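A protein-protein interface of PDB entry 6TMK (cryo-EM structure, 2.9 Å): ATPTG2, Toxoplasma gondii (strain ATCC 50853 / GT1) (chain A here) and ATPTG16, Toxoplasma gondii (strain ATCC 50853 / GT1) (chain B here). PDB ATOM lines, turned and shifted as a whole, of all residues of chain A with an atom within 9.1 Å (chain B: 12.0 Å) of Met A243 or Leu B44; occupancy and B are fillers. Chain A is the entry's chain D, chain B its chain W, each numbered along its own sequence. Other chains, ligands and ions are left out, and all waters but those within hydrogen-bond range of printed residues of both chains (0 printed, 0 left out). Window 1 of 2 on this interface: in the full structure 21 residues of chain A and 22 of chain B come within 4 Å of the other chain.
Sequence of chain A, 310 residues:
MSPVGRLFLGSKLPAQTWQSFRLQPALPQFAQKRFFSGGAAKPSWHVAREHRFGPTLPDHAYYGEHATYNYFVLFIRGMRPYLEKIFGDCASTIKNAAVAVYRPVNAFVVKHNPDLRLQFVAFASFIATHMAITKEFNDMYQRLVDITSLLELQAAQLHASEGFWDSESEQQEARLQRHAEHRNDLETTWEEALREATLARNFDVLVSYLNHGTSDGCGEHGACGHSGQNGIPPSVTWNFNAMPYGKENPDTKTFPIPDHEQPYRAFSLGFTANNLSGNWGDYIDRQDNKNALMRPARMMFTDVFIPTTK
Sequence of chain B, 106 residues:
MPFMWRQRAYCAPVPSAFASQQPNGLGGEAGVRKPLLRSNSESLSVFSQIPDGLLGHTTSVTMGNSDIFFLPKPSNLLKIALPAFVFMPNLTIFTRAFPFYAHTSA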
ATOM      1  N   HIS A 159     -35.582  24.427  10.760  1.00  0.00           N
ATOM      2  CA  HIS A 159     -35.082  24.969   9.503  1.00  0.00           C
ATOM      3  C   HIS A 159     -35.917  26.141   9.020  1.00  0.00           C
ATOM      4  O   HIS A 159     -35.379  27.082   8.428  1.00  0.00           O
ATOM      5  CB  HIS A 159     -35.073  23.890   8.427  1.00  0.00           C
ATOM      6  CG  HIS A 159     -33.859  23.025   8.433  1.00  0.00           C
ATOM      7  ND1 HIS A 159     -33.916  21.669   8.203  1.00  0.00           N
ATOM      8  CD2 HIS A 159     -32.550  23.324   8.601  1.00  0.00           C
ATOM      9  CE1 HIS A 159     -32.697  21.166   8.250  1.00  0.00           C
ATOM     10  NE2 HIS A 159     -31.850  22.151   8.488  1.00  0.00           N
ATOM     11  N   PHE A 164     -34.587  28.464   5.972  1.00  0.00           N
ATOM     12  CA  PHE A 164     -33.930  27.522   5.081  1.00  0.00           C
ATOM     13  C   PHE A 164     -34.832  27.123   3.923  1.00  0.00           C
ATOM     14  O   PHE A 164     -34.355  26.933   2.802  1.00  0.00           O
ATOM     15  CB  PHE A 164     -33.487  26.306   5.881  1.00  0.00           C
ATOM     16  CG  PHE A 164     -32.607  25.378   5.132  1.00  0.00           C
ATOM     17  CD1 PHE A 164     -31.304  25.707   4.867  1.00  0.00           C
ATOM     18  CD2 PHE A 164     -33.075  24.154   4.725  1.00  0.00           C
ATOM     19  CE1 PHE A 164     -30.500  24.851   4.189  1.00  0.00           C
ATOM     20  CE2 PHE A 164     -32.268  23.293   4.052  1.00  0.00           C
ATOM     21  CZ  PHE A 164     -30.979  23.640   3.786  1.00  0.00           C
ATOM     22  N   TRP A 165     -36.130  27.007   4.168  1.00  0.00           N
ATOM     23  CA  TRP A 165     -37.072  26.703   3.106  1.00  0.00           C
ATOM     24  C   TRP A 165     -37.421  27.922   2.269  1.00  0.00           C
ATOM     25  O   TRP A 165     -38.012  27.766   1.196  1.00  0.00           O
ATOM     26  CB  TRP A 165     -38.351  26.116   3.693  1.00  0.00           C
ATOM     27  CG  TRP A 165     -38.156  24.947   4.594  1.00  0.00           C
ATOM     28  CD1 TRP A 165     -38.685  24.786   5.829  1.00  0.00           C
ATOM     29  CD2 TRP A 165     -37.394  23.767   4.330  1.00  0.00           C
ATOM     30  NE1 TRP A 165     -38.299  23.589   6.361  1.00  0.00           N
ATOM     31  CE2 TRP A 165     -37.505  22.942   5.457  1.00  0.00           C
ATOM     32  CE3 TRP A 165     -36.631  23.326   3.252  1.00  0.00           C
ATOM     33  CZ2 TRP A 165     -36.882  21.710   5.538  1.00  0.00           C
ATOM     34  CZ3 TRP A 165     -36.014  22.107   3.341  1.00  0.00           C
ATOM     35  CH2 TRP A 165     -36.144  21.314   4.473  1.00  0.00           C
ATOM     36  N   GLU A 168     -34.382  32.928  -2.195  1.00  0.00           N
ATOM     37  CA  GLU A 168     -33.493  34.078  -2.087  1.00  0.00           C
ATOM     38  C   GLU A 168     -34.254  35.389  -2.213  1.00  0.00           C
ATOM     39  O   GLU A 168     -33.888  36.380  -1.574  1.00  0.00           O
ATOM     40  CB  GLU A 168     -32.396  33.995  -3.140  1.00  0.00           C
ATOM     41  CG  GLU A 168     -31.158  34.793  -2.770  1.00  0.00           C
ATOM     42  CD  GLU A 168     -30.407  34.189  -1.607  1.00  0.00           C
ATOM     43  OE1 GLU A 168     -30.124  32.974  -1.652  1.00  0.00           O
ATOM     44  OE2 GLU A 168     -30.112  34.924  -0.639  1.00  0.00           O
ATOM     45  N   TRP A 238     -28.000  30.943   3.863  1.00  0.00           N
ATOM     46  CA  TRP A 238     -28.016  29.724   3.077  1.00  0.00           C
ATOM     47  C   TRP A 238     -29.431  29.181   3.051  1.00  0.00           C
ATOM     48  O   TRP A 238     -30.165  29.292   4.037  1.00  0.00           O
ATOM     49  CB  TRP A 238     -27.067  28.699   3.671  1.00  0.00           C
ATOM     50  CG  TRP A 238     -26.909  27.446   2.887  1.00  0.00           C
ATOM     51  CD1 TRP A 238     -27.243  26.196   3.286  1.00  0.00           C
ATOM     52  CD2 TRP A 238     -26.347  27.311   1.580  1.00  0.00           C
ATOM     53  NE1 TRP A 238     -26.938  25.290   2.314  1.00  0.00           N
ATOM     54  CE2 TRP A 238     -26.385  25.950   1.252  1.00  0.00           C
ATOM     55  CE3 TRP A 238     -25.818  28.211   0.656  1.00  0.00           C
ATOM     56  CZ2 TRP A 238     -25.920  25.465   0.038  1.00  0.00           C
ATOM     57  CZ3 TRP A 238     -25.358  27.724  -0.547  1.00  0.00           C
ATOM     58  CH2 TRP A 238     -25.412  26.366  -0.844  1.00  0.00           C
ATOM     59  N   ASN A 239     -29.819  28.604   1.921  1.00  0.00           N
ATOM     60  CA  ASN A 239     -31.169  28.112   1.738  1.00  0.00           C
ATOM     61  C   ASN A 239     -31.116  26.750   1.071  1.00  0.00           C
ATOM     62  O   ASN A 239     -30.054  26.261   0.678  1.00  0.00           O
ATOM     63  CB  ASN A 239     -32.005  29.056   0.878  1.00  0.00           C
ATOM     64  CG  ASN A 239     -31.364  29.330  -0.444  1.00  0.00           C
ATOM     65  OD1 ASN A 239     -30.260  28.870  -0.715  1.00  0.00           O
ATOM     66  ND2 ASN A 239     -32.059  30.043  -1.291  1.00  0.00           N
ATOM     67  N   PHE A 240     -32.292  26.156   0.924  1.00  0.00           N
ATOM     68  CA  PHE A 240     -32.416  24.829   0.354  1.00  0.00           C
ATOM     69  C   PHE A 240     -32.324  24.854  -1.164  1.00  0.00           C
ATOM     70  O   PHE A 240     -31.850  23.886  -1.767  1.00  0.00           O
ATOM     71  CB  PHE A 240     -33.739  24.223   0.808  1.00  0.00           C
ATOM     72  CG  PHE A 240     -34.123  22.985   0.086  1.00  0.00           C
ATOM     73  CD1 PHE A 240     -33.377  21.835   0.199  1.00  0.00           C
ATOM     74  CD2 PHE A 240     -35.246  22.971  -0.701  1.00  0.00           C
ATOM     75  CE1 PHE A 240     -33.747  20.704  -0.470  1.00  0.00           C
ATOM     76  CE2 PHE A 240     -35.617  21.843  -1.368  1.00  0.00           C
ATOM     77  CZ  PHE A 240     -34.867  20.710  -1.253  1.00  0.00           C
ATOM     78  N   ASN A 241     -32.754  25.942  -1.796  1.00  0.00           N
ATOM     79  CA  ASN A 241     -32.724  26.035  -3.247  1.00  0.00           C
ATOM     80  C   ASN A 241     -31.338  26.306  -3.794  1.00  0.00           C
ATOM     81  O   ASN A 241     -31.153  26.259  -5.013  1.00  0.00           O
ATOM     82  CB  ASN A 241     -33.661  27.126  -3.742  1.00  0.00           C
ATOM     83  CG  ASN A 241     -35.109  26.740  -3.649  1.00  0.00           C
ATOM     84  OD1 ASN A 241     -35.457  25.563  -3.580  1.00  0.00           O
ATOM     85  ND2 ASN A 241     -35.969  27.734  -3.674  1.00  0.00           N
ATOM     86  N   ALA A 242     -30.365  26.584  -2.934  1.00  0.00           N
ATOM     87  CA  ALA A 242     -28.995  26.718  -3.385  1.00  0.00           C
ATOM     88  C   ALA A 242     -28.286  25.377  -3.470  1.00  0.00           C
ATOM     89  O   ALA A 242     -27.224  25.293  -4.092  1.00  0.00           O
ATOM     90  CB  ALA A 242     -28.239  27.657  -2.450  1.00  0.00           C
ATOM     91  N   MET A 243     -28.835  24.344  -2.853  1.00  0.00           N
ATOM     92  CA  MET A 243     -28.275  23.013  -2.993  1.00  0.00           C
ATOM     93  C   MET A 243     -28.602  22.488  -4.385  1.00  0.00           C
ATOM     94  O   MET A 243     -29.757  22.574  -4.815  1.00  0.00           O
ATOM     95  CB  MET A 243     -28.825  22.082  -1.919  1.00  0.00           C
ATOM     96  CG  MET A 243     -28.447  22.477  -0.517  1.00  0.00           C
ATOM     97  SD  MET A 243     -28.744  21.193   0.712  1.00  0.00           S
ATOM     98  CE  MET A 243     -27.875  21.867   2.135  1.00  0.00           C
ATOM     99  N   PRO A 244     -27.636  21.958  -5.122  1.00  0.00           N
ATOM    100  CA  PRO A 244     -27.920  21.523  -6.486  1.00  0.00           C
ATOM    101  C   PRO A 244     -28.592  20.162  -6.537  1.00  0.00           C
ATOM    102  O   PRO A 244     -28.493  19.343  -5.623  1.00  0.00           O
ATOM    103  CB  PRO A 244     -26.530  21.472  -7.121  1.00  0.00           C
ATOM    104  CG  PRO A 244     -25.649  21.127  -6.005  1.00  0.00           C
ATOM    105  CD  PRO A 244     -26.204  21.844  -4.814  1.00  0.00           C
ATOM    106  N   TYR A 245     -29.288  19.937  -7.645  1.00  0.00           N
ATOM    107  CA  TYR A 245     -29.931  18.668  -7.925  1.00  0.00           C
ATOM    108  C   TYR A 245     -29.870  18.384  -9.412  1.00  0.00           C
ATOM    109  O   TYR A 245     -30.029  19.289 -10.232  1.00  0.00           O
ATOM    110  CB  TYR A 245     -31.387  18.653  -7.462  1.00  0.00           C
ATOM    111  CG  TYR A 245     -32.025  17.302  -7.546  1.00  0.00           C
ATOM    112  CD1 TYR A 245     -32.936  17.009  -8.540  1.00  0.00           C
ATOM    113  CD2 TYR A 245     -31.718  16.316  -6.632  1.00  0.00           C
ATOM    114  CE1 TYR A 245     -33.517  15.778  -8.623  1.00  0.00           C
ATOM    115  CE2 TYR A 245     -32.297  15.080  -6.708  1.00  0.00           C
ATOM    116  CZ  TYR A 245     -33.198  14.816  -7.703  1.00  0.00           C
ATOM    117  OH  TYR A 245     -33.778  13.580  -7.774  1.00  0.00           O
ATOM    118  N   GLY A 246     -29.648  17.123  -9.752  1.00  0.00           N
ATOM    119  CA  GLY A 246     -29.723  16.700 -11.130  1.00  0.00           C
ATOM    120  C   GLY A 246     -28.974  15.425 -11.412  1.00  0.00           C
ATOM    121  O   GLY A 246     -27.863  15.222 -10.919  1.00  0.00           O
ATOM    122  N   ASN A 249     -26.666  17.089 -13.911  1.00  0.00           N
ATOM    123  CA  ASN A 249     -26.091  18.355 -13.484  1.00  0.00           C
ATOM    124  C   ASN A 249     -24.678  18.148 -12.962  1.00  0.00           C
ATOM    125  O   ASN A 249     -24.492  17.398 -11.995  1.00  0.00           O
ATOM    126  CB  ASN A 249     -26.966  18.982 -12.417  1.00  0.00           C
ATOM    127  CG  ASN A 249     -26.551  20.388 -12.078  1.00  0.00           C
ATOM    128  OD1 ASN A 249     -25.738  20.998 -12.769  1.00  0.00           O
ATOM    129  ND2 ASN A 249     -27.121  20.918 -11.012  1.00  0.00           N
ATOM    130  N   ASP A 251     -22.913  20.145 -11.253  1.00  0.00           N
ATOM    131  CA  ASP A 251     -22.708  20.769  -9.954  1.00  0.00           C
ATOM    132  C   ASP A 251     -22.800  19.763  -8.821  1.00  0.00           C
ATOM    133  O   ASP A 251     -22.572  20.129  -7.664  1.00  0.00           O
ATOM    134  CB  ASP A 251     -23.721  21.892  -9.735  1.00  0.00           C
ATOM    135  CG  ASP A 251     -23.685  22.936 -10.832  1.00  0.00           C
ATOM    136  OD1 ASP A 251     -22.822  22.836 -11.731  1.00  0.00           O
ATOM    137  OD2 ASP A 251     -24.517  23.865 -10.793  1.00  0.00           O
ATOM    138  N   THR A 252     -23.117  18.510  -9.136  1.00  0.00           N
ATOM    139  CA  THR A 252     -23.174  17.429  -8.167  1.00  0.00           C
ATOM    140  C   THR A 252     -22.095  16.378  -8.361  1.00  0.00           C
ATOM    141  O   THR A 252     -21.965  15.491  -7.514  1.00  0.00           O
ATOM    142  CB  THR A 252     -24.542  16.741  -8.238  1.00  0.00           C
ATOM    143  OG1 THR A 252     -24.833  16.405  -9.599  1.00  0.00           O
ATOM    144  CG2 THR A 252     -25.620  17.631  -7.719  1.00  0.00           C
ATOM    145  N   ILE A 284     -38.133  14.417  -7.716  1.00  0.00           N
ATOM    146  CA  ILE A 284     -38.158  15.868  -7.812  1.00  0.00           C
ATOM    147  C   ILE A 284     -38.354  16.246  -9.267  1.00  0.00           C
ATOM    148  O   ILE A 284     -39.297  16.962  -9.619  1.00  0.00           O
ATOM    149  CB  ILE A 284     -36.870  16.491  -7.245  1.00  0.00           C
ATOM    150  CG1 ILE A 284     -36.507  15.840  -5.916  1.00  0.00           C
ATOM    151  CG2 ILE A 284     -37.013  17.982  -7.101  1.00  0.00           C
ATOM    152  CD1 ILE A 284     -35.389  16.517  -5.196  1.00  0.00           C
ATOM    153  N   ARG B   8     -18.712  31.872   1.370  1.00  0.00           N
ATOM    154  CA  ARG B   8     -19.079  30.506   1.712  1.00  0.00           C
ATOM    155  C   ARG B   8     -20.136  30.587   2.808  1.00  0.00           C
ATOM    156  O   ARG B   8     -19.820  30.634   3.997  1.00  0.00           O
ATOM    157  CB  ARG B   8     -17.862  29.724   2.148  1.00  0.00           C
ATOM    158  CG  ARG B   8     -16.842  29.519   1.067  1.00  0.00           C
ATOM    159  CD  ARG B   8     -15.479  29.219   1.631  1.00  0.00           C
ATOM    160  NE  ARG B   8     -15.324  27.820   2.010  1.00  0.00           N
ATOM    161  CZ  ARG B   8     -14.861  27.392   3.178  1.00  0.00           C
ATOM    162  NH1 ARG B   8     -14.501  28.240   4.129  1.00  0.00           N
ATOM    163  NH2 ARG B   8     -14.765  26.095   3.394  1.00  0.00           N
ATOM    164  N   ALA B   9     -21.400  30.615   2.395  1.00  0.00           N
ATOM    165  CA  ALA B   9     -22.499  30.701   3.341  1.00  0.00           C
ATOM    166  C   ALA B   9     -22.878  29.350   3.921  1.00  0.00           C
ATOM    167  O   ALA B   9     -23.454  29.295   5.011  1.00  0.00           O
ATOM    168  CB  ALA B   9     -23.707  31.336   2.669  1.00  0.00           C
ATOM    169  N   TYR B  10     -22.580  28.264   3.210  1.00  0.00           N
ATOM    170  CA  TYR B  10     -22.883  26.935   3.723  1.00  0.00           C
ATOM    171  C   TYR B  10     -22.118  26.632   5.004  1.00  0.00           C
ATOM    172  O   TYR B  10     -22.606  25.874   5.849  1.00  0.00           O
ATOM    173  CB  TYR B  10     -22.600  25.881   2.656  1.00  0.00           C
ATOM    174  CG  TYR B  10     -21.298  26.035   1.916  1.00  0.00           C
ATOM    175  CD1 TYR B  10     -20.098  25.714   2.511  1.00  0.00           C
ATOM    176  CD2 TYR B  10     -21.274  26.498   0.616  1.00  0.00           C
ATOM    177  CE1 TYR B  10     -18.919  25.856   1.841  1.00  0.00           C
ATOM    178  CE2 TYR B  10     -20.098  26.638  -0.062  1.00  0.00           C
ATOM    179  CZ  TYR B  10     -18.919  26.310   0.553  1.00  0.00           C
ATOM    180  OH  TYR B  10     -17.735  26.450  -0.120  1.00  0.00           O
ATOM    181  N   CYS B  11     -20.927  27.200   5.172  1.00  0.00           N
ATOM    182  CA  CYS B  11     -20.099  26.940   6.340  1.00  0.00           C
ATOM    183  C   CYS B  11     -20.265  28.012   7.411  1.00  0.00           C
ATOM    184  O   CYS B  11     -19.391  28.165   8.271  1.00  0.00           O
ATOM    185  CB  CYS B  11     -18.631  26.827   5.937  1.00  0.00           C
ATOM    186  SG  CYS B  11     -17.864  28.372   5.464  1.00  0.00           S
ATOM    187  N   ALA B  12     -21.365  28.742   7.381  1.00  0.00           N
ATOM    188  CA  ALA B  12     -21.588  29.892   8.230  1.00  0.00           C
ATOM    189  C   ALA B  12     -22.593  29.569   9.324  1.00  0.00           C
ATOM    190  O   ALA B  12     -23.361  28.609   9.216  1.00  0.00           O
ATOM    191  CB  ALA B  12     -22.098  31.079   7.410  1.00  0.00           C
ATOM    192  N   VAL B  14     -25.960  29.871  11.709  1.00  0.00           N
ATOM    193  CA  VAL B  14     -27.367  30.094  11.420  1.00  0.00           C
ATOM    194  C   VAL B  14     -27.756  31.477  11.925  1.00  0.00           C
ATOM    195  O   VAL B  14     -27.078  32.032  12.798  1.00  0.00           O
ATOM    196  CB  VAL B  14     -28.238  28.993  12.040  1.00  0.00           C
ATOM    197  CG1 VAL B  14     -27.773  27.646  11.559  1.00  0.00           C
ATOM    198  CG2 VAL B  14     -28.194  29.052  13.548  1.00  0.00           C
ATOM    199  N   ARG B  38     -24.543  27.079  15.937  1.00  0.00           N
ATOM    200  CA  ARG B  38     -24.758  25.997  14.992  1.00  0.00           C
ATOM    201  C   ARG B  38     -24.449  26.501  13.593  1.00  0.00           C
ATOM    202  O   ARG B  38     -24.634  27.681  13.285  1.00  0.00           O
ATOM    203  CB  ARG B  38     -26.186  25.455  15.056  1.00  0.00           C
ATOM    204  CG  ARG B  38     -26.593  25.004  16.433  1.00  0.00           C
ATOM    205  CD  ARG B  38     -27.906  24.259  16.422  1.00  0.00           C
ATOM    206  NE  ARG B  38     -28.986  25.076  15.879  1.00  0.00           N
ATOM    207  CZ  ARG B  38     -29.446  24.990  14.636  1.00  0.00           C
ATOM    208  NH1 ARG B  38     -28.934  24.122  13.777  1.00  0.00           N
ATOM    209  NH2 ARG B  38     -30.425  25.785  14.249  1.00  0.00           N
ATOM    210  N   SER B  39     -23.962  25.599  12.755  1.00  0.00           N
ATOM    211  CA  SER B  39     -23.589  25.920  11.390  1.00  0.00           C
ATOM    212  C   SER B  39     -24.688  25.513  10.419  1.00  0.00           C
ATOM    213  O   SER B  39     -25.580  24.727  10.741  1.00  0.00           O
ATOM    214  CB  SER B  39     -22.289  25.207  11.024  1.00  0.00           C
ATOM    215  OG  SER B  39     -21.842  25.539   9.730  1.00  0.00           O
ATOM    216  N   ASN B  40     -24.609  26.070   9.213  1.00  0.00           N
ATOM    217  CA  ASN B  40     -25.451  25.621   8.116  1.00  0.00           C
ATOM    218  C   ASN B  40     -24.918  24.357   7.459  1.00  0.00           C
ATOM    219  O   ASN B  40     -25.657  23.697   6.723  1.00  0.00           O
ATOM    220  CB  ASN B  40     -25.587  26.730   7.077  1.00  0.00           C
ATOM    221  CG  ASN B  40     -26.614  27.761   7.461  1.00  0.00           C
ATOM    222  OD1 ASN B  40     -27.708  27.429   7.910  1.00  0.00           O
ATOM    223  ND2 ASN B  40     -26.270  29.024   7.284  1.00  0.00           N
ATOM    224  N   SER B  41     -23.658  24.007   7.713  1.00  0.00           N
ATOM    225  CA  SER B  41     -23.068  22.790   7.181  1.00  0.00           C
ATOM    226  C   SER B  41     -23.656  21.541   7.810  1.00  0.00           C
ATOM    227  O   SER B  41     -23.433  20.440   7.296  1.00  0.00           O
ATOM    228  CB  SER B  41     -21.559  22.823   7.394  1.00  0.00           C
ATOM    229  OG  SER B  41     -21.242  22.878   8.767  1.00  0.00           O
ATOM    230  N   GLU B  42     -24.395  21.686   8.905  1.00  0.00           N
ATOM    231  CA  GLU B  42     -25.108  20.565   9.488  1.00  0.00           C
ATOM    232  C   GLU B  42     -26.263  20.102   8.616  1.00  0.00           C
ATOM    233  O   GLU B  42     -26.761  18.990   8.808  1.00  0.00           O
ATOM    234  CB  GLU B  42     -25.634  20.983  10.851  1.00  0.00           C
ATOM    235  CG  GLU B  42     -24.597  20.965  11.940  1.00  0.00           C
ATOM    236  CD  GLU B  42     -25.205  21.023  13.321  1.00  0.00           C
ATOM    237  OE1 GLU B  42     -26.442  21.172  13.424  1.00  0.00           O
ATOM    238  OE2 GLU B  42     -24.446  20.930  14.306  1.00  0.00           O
ATOM    239  N   SER B  43     -26.690  20.927   7.662  1.00  0.00           N
ATOM    240  CA  SER B  43     -27.711  20.514   6.712  1.00  0.00           C
ATOM    241  C   SER B  43     -27.234  19.381   5.818  1.00  0.00           C
ATOM    242  O   SER B  43     -28.060  18.680   5.229  1.00  0.00           O
ATOM    243  CB  SER B  43     -28.121  21.710   5.858  1.00  0.00           C
ATOM    244  OG  SER B  43     -28.694  22.721   6.659  1.00  0.00           O
ATOM    245  N   LEU B  44     -25.924  19.187   5.711  1.00  0.00           N
ATOM    246  CA  LEU B  44     -25.362  18.119   4.899  1.00  0.00           C
ATOM    247  C   LEU B  44     -25.305  16.786   5.621  1.00  0.00           C
ATOM    248  O   LEU B  44     -24.793  15.817   5.052  1.00  0.00           O
ATOM    249  CB  LEU B  44     -23.969  18.505   4.416  1.00  0.00           C
ATOM    250  CG  LEU B  44     -23.898  19.813   3.641  1.00  0.00           C
ATOM    251  CD1 LEU B  44     -22.472  20.178   3.391  1.00  0.00           C
ATOM    252  CD2 LEU B  44     -24.646  19.695   2.341  1.00  0.00           C
ATOM    253  N   SER B  45     -25.792  16.713   6.852  1.00  0.00           N
ATOM    254  CA  SER B  45     -25.868  15.465   7.585  1.00  0.00           C
ATOM    255  C   SER B  45     -27.326  15.129   7.843  1.00  0.00           C
ATOM    256  O   SER B  45     -28.158  16.013   8.063  1.00  0.00           O
ATOM    257  CB  SER B  45     -25.105  15.546   8.907  1.00  0.00           C
ATOM    258  OG  SER B  45     -23.716  15.694   8.686  1.00  0.00           O
ATOM    259  N   VAL B  46     -27.625  13.835   7.817  1.00  0.00           N
ATOM    260  CA  VAL B  46     -28.994  13.382   8.025  1.00  0.00           C
ATOM    261  C   VAL B  46     -29.345  13.400   9.505  1.00  0.00           C
ATOM    262  O   VAL B  46     -30.312  14.043   9.926  1.00  0.00           O
ATOM    263  CB  VAL B  46     -29.190  11.984   7.413  1.00  0.00           C
ATOM    264  CG1 VAL B  46     -30.469  11.363   7.890  1.00  0.00           C
ATOM    265  CG2 VAL B  46     -29.190  12.078   5.919  1.00  0.00           C
ATOM    266  N   PHE B  47     -28.565  12.687  10.316  1.00  0.00           N
ATOM    267  CA  PHE B  47     -28.877  12.493  11.724  1.00  0.00           C
ATOM    268  C   PHE B  47     -28.226  13.541  12.613  1.00  0.00           C
ATOM    269  O   PHE B  47     -27.932  13.265  13.782  1.00  0.00           O
ATOM    270  CB  PHE B  47     -28.460  11.089  12.155  1.00  0.00           C
ATOM    271  CG  PHE B  47     -29.278  10.008  11.530  1.00  0.00           C
ATOM    272  CD1 PHE B  47     -28.748   9.231  10.527  1.00  0.00           C
ATOM    273  CD2 PHE B  47     -30.581   9.787  11.923  1.00  0.00           C
ATOM    274  CE1 PHE B  47     -29.493   8.244   9.937  1.00  0.00           C
ATOM    275  CE2 PHE B  47     -31.331   8.800  11.337  1.00  0.00           C
ATOM    276  CZ  PHE B  47     -30.788   8.029  10.339  1.00  0.00           C
ATOM    277  N   SER B  48     -27.991  14.742  12.087  1.00  0.00           N
ATOM    278  CA  SER B  48     -27.486  15.830  12.913  1.00  0.00           C
ATOM    279  C   SER B  48     -28.480  16.200  14.004  1.00  0.00           C
ATOM    280  O   SER B  48     -28.194  16.071  15.199  1.00  0.00           O
ATOM    281  CB  SER B  48     -27.179  17.043  12.038  1.00  0.00           C
ATOM    282  OG  SER B  48     -28.370  17.575  11.493  1.00  0.00           O
ATOM    283  N   GLN B  49     -29.662  16.662  13.607  1.00  0.00           N
ATOM    284  CA  GLN B  49     -30.665  17.098  14.567  1.00  0.00           C
ATOM    285  C   GLN B  49     -31.653  15.994  14.913  1.00  0.00           C
ATOM    286  O   GLN B  49     -31.993  15.817  16.087  1.00  0.00           O
ATOM    287  CB  GLN B  49     -31.414  18.316  14.024  1.00  0.00           C
ATOM    288  CG  GLN B  49     -32.421  18.920  14.997  1.00  0.00           C
ATOM    289  CD  GLN B  49     -31.796  19.320  16.319  1.00  0.00           C
ATOM    290  OE1 GLN B  49     -31.442  20.481  16.525  1.00  0.00           O
ATOM    291  NE2 GLN B  49     -31.657  18.358  17.225  1.00  0.00           N
ATOM    292  N   ILE B  50     -32.123  15.246  13.922  1.00  0.00           N
ATOM    293  CA  ILE B  50     -33.047  14.147  14.181  1.00  0.00           C
ATOM    294  C   ILE B  50     -32.279  13.034  14.878  1.00  0.00           C
ATOM    295  O   ILE B  50     -31.055  12.931  14.717  1.00  0.00           O
ATOM    296  CB  ILE B  50     -33.701  13.628  12.893  1.00  0.00           C
ATOM    297  CG1 ILE B  50     -32.649  13.099  11.926  1.00  0.00           C
ATOM    298  CG2 ILE B  50     -34.468  14.735  12.217  1.00  0.00           C
ATOM    299  CD1 ILE B  50     -33.226  12.300  10.801  1.00  0.00           C
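N of Phe A164 sits at hydrogen-bond distance from O of His A159 (2.9 Å). O of Phe A164 is in hydrogen-bond range of N of Phe A240 (2.9 Å). The backbone carbonyl oxygen (O) of Ala B12 is in hydrogen-bond range of the backbone NH (N) of Asn B40, at 2.8 Å. The backbone carbonyl oxygen (O) of Asn B40 is in hydrogen-bond range of the side-chain hydroxyl (OG) of Ser B43, 3.2 Å away.
Among the printed residues, pairs that only touch across the chains: His A159 with Ser B43 (3.7 Å), Trp A238 with Asn B40 (3.7 Å), Phe A164 with Ser B43 (3.7 Å), Met A243 with Ser B43 (3.7 Å), Met A243 with Leu B44 (3.9 Å) and Trp A238 with Ala B9 (3.9 Å).
Met A243 touches just these residues of chain B: Ser B43 (3.7 Å) and Leu B44 (3.9 Å). Leu B44 touches just one residue of chain A: Met A243 (3.9 Å). No residue of chain B comes within 4 Å of Phe A240. Ser B43 touches three residues of chain A. No residue of chain A comes within 4 Å of Ser B45. Of the printed residues of chain B, Phe A164 touches Ser B43. Of the printed residues of chain B, Trp A238 touches Ala B9 (3.9 Å) and Asn B40 (3.7 Å). Of the printed residues of chain B, His A159 touches Ser B43. Of the printed residues of chain A, Asn B40 touches Trp A238. Printed residues of chain A within 4 Å of Ala B9: Trp A238. The nearest residue of chain B that does not touch Met A243 is Asn B40 (5.4 Å).
Of the 17 printed residues of chain A, 4 touch a printed residue of chain B. Printed residues of chain A that touch a printed residue of chain B: His A159, Phe A164, Trp A238 and Met A243. Of the 19 printed residues of chain B, 4 touch a printed residue of chain A. Hydrophobic or aromatic side chains of chain B within 4 Å of the printed part of chain A: Leu B44. Along chain B the printed residues that touch a printed residue of chain A span positions 9 to 44. Among the printed residues, no Asp or Glu carboxylate lies within 4 Å of a Lys or Arg side-chain nitrogen of the other chain.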
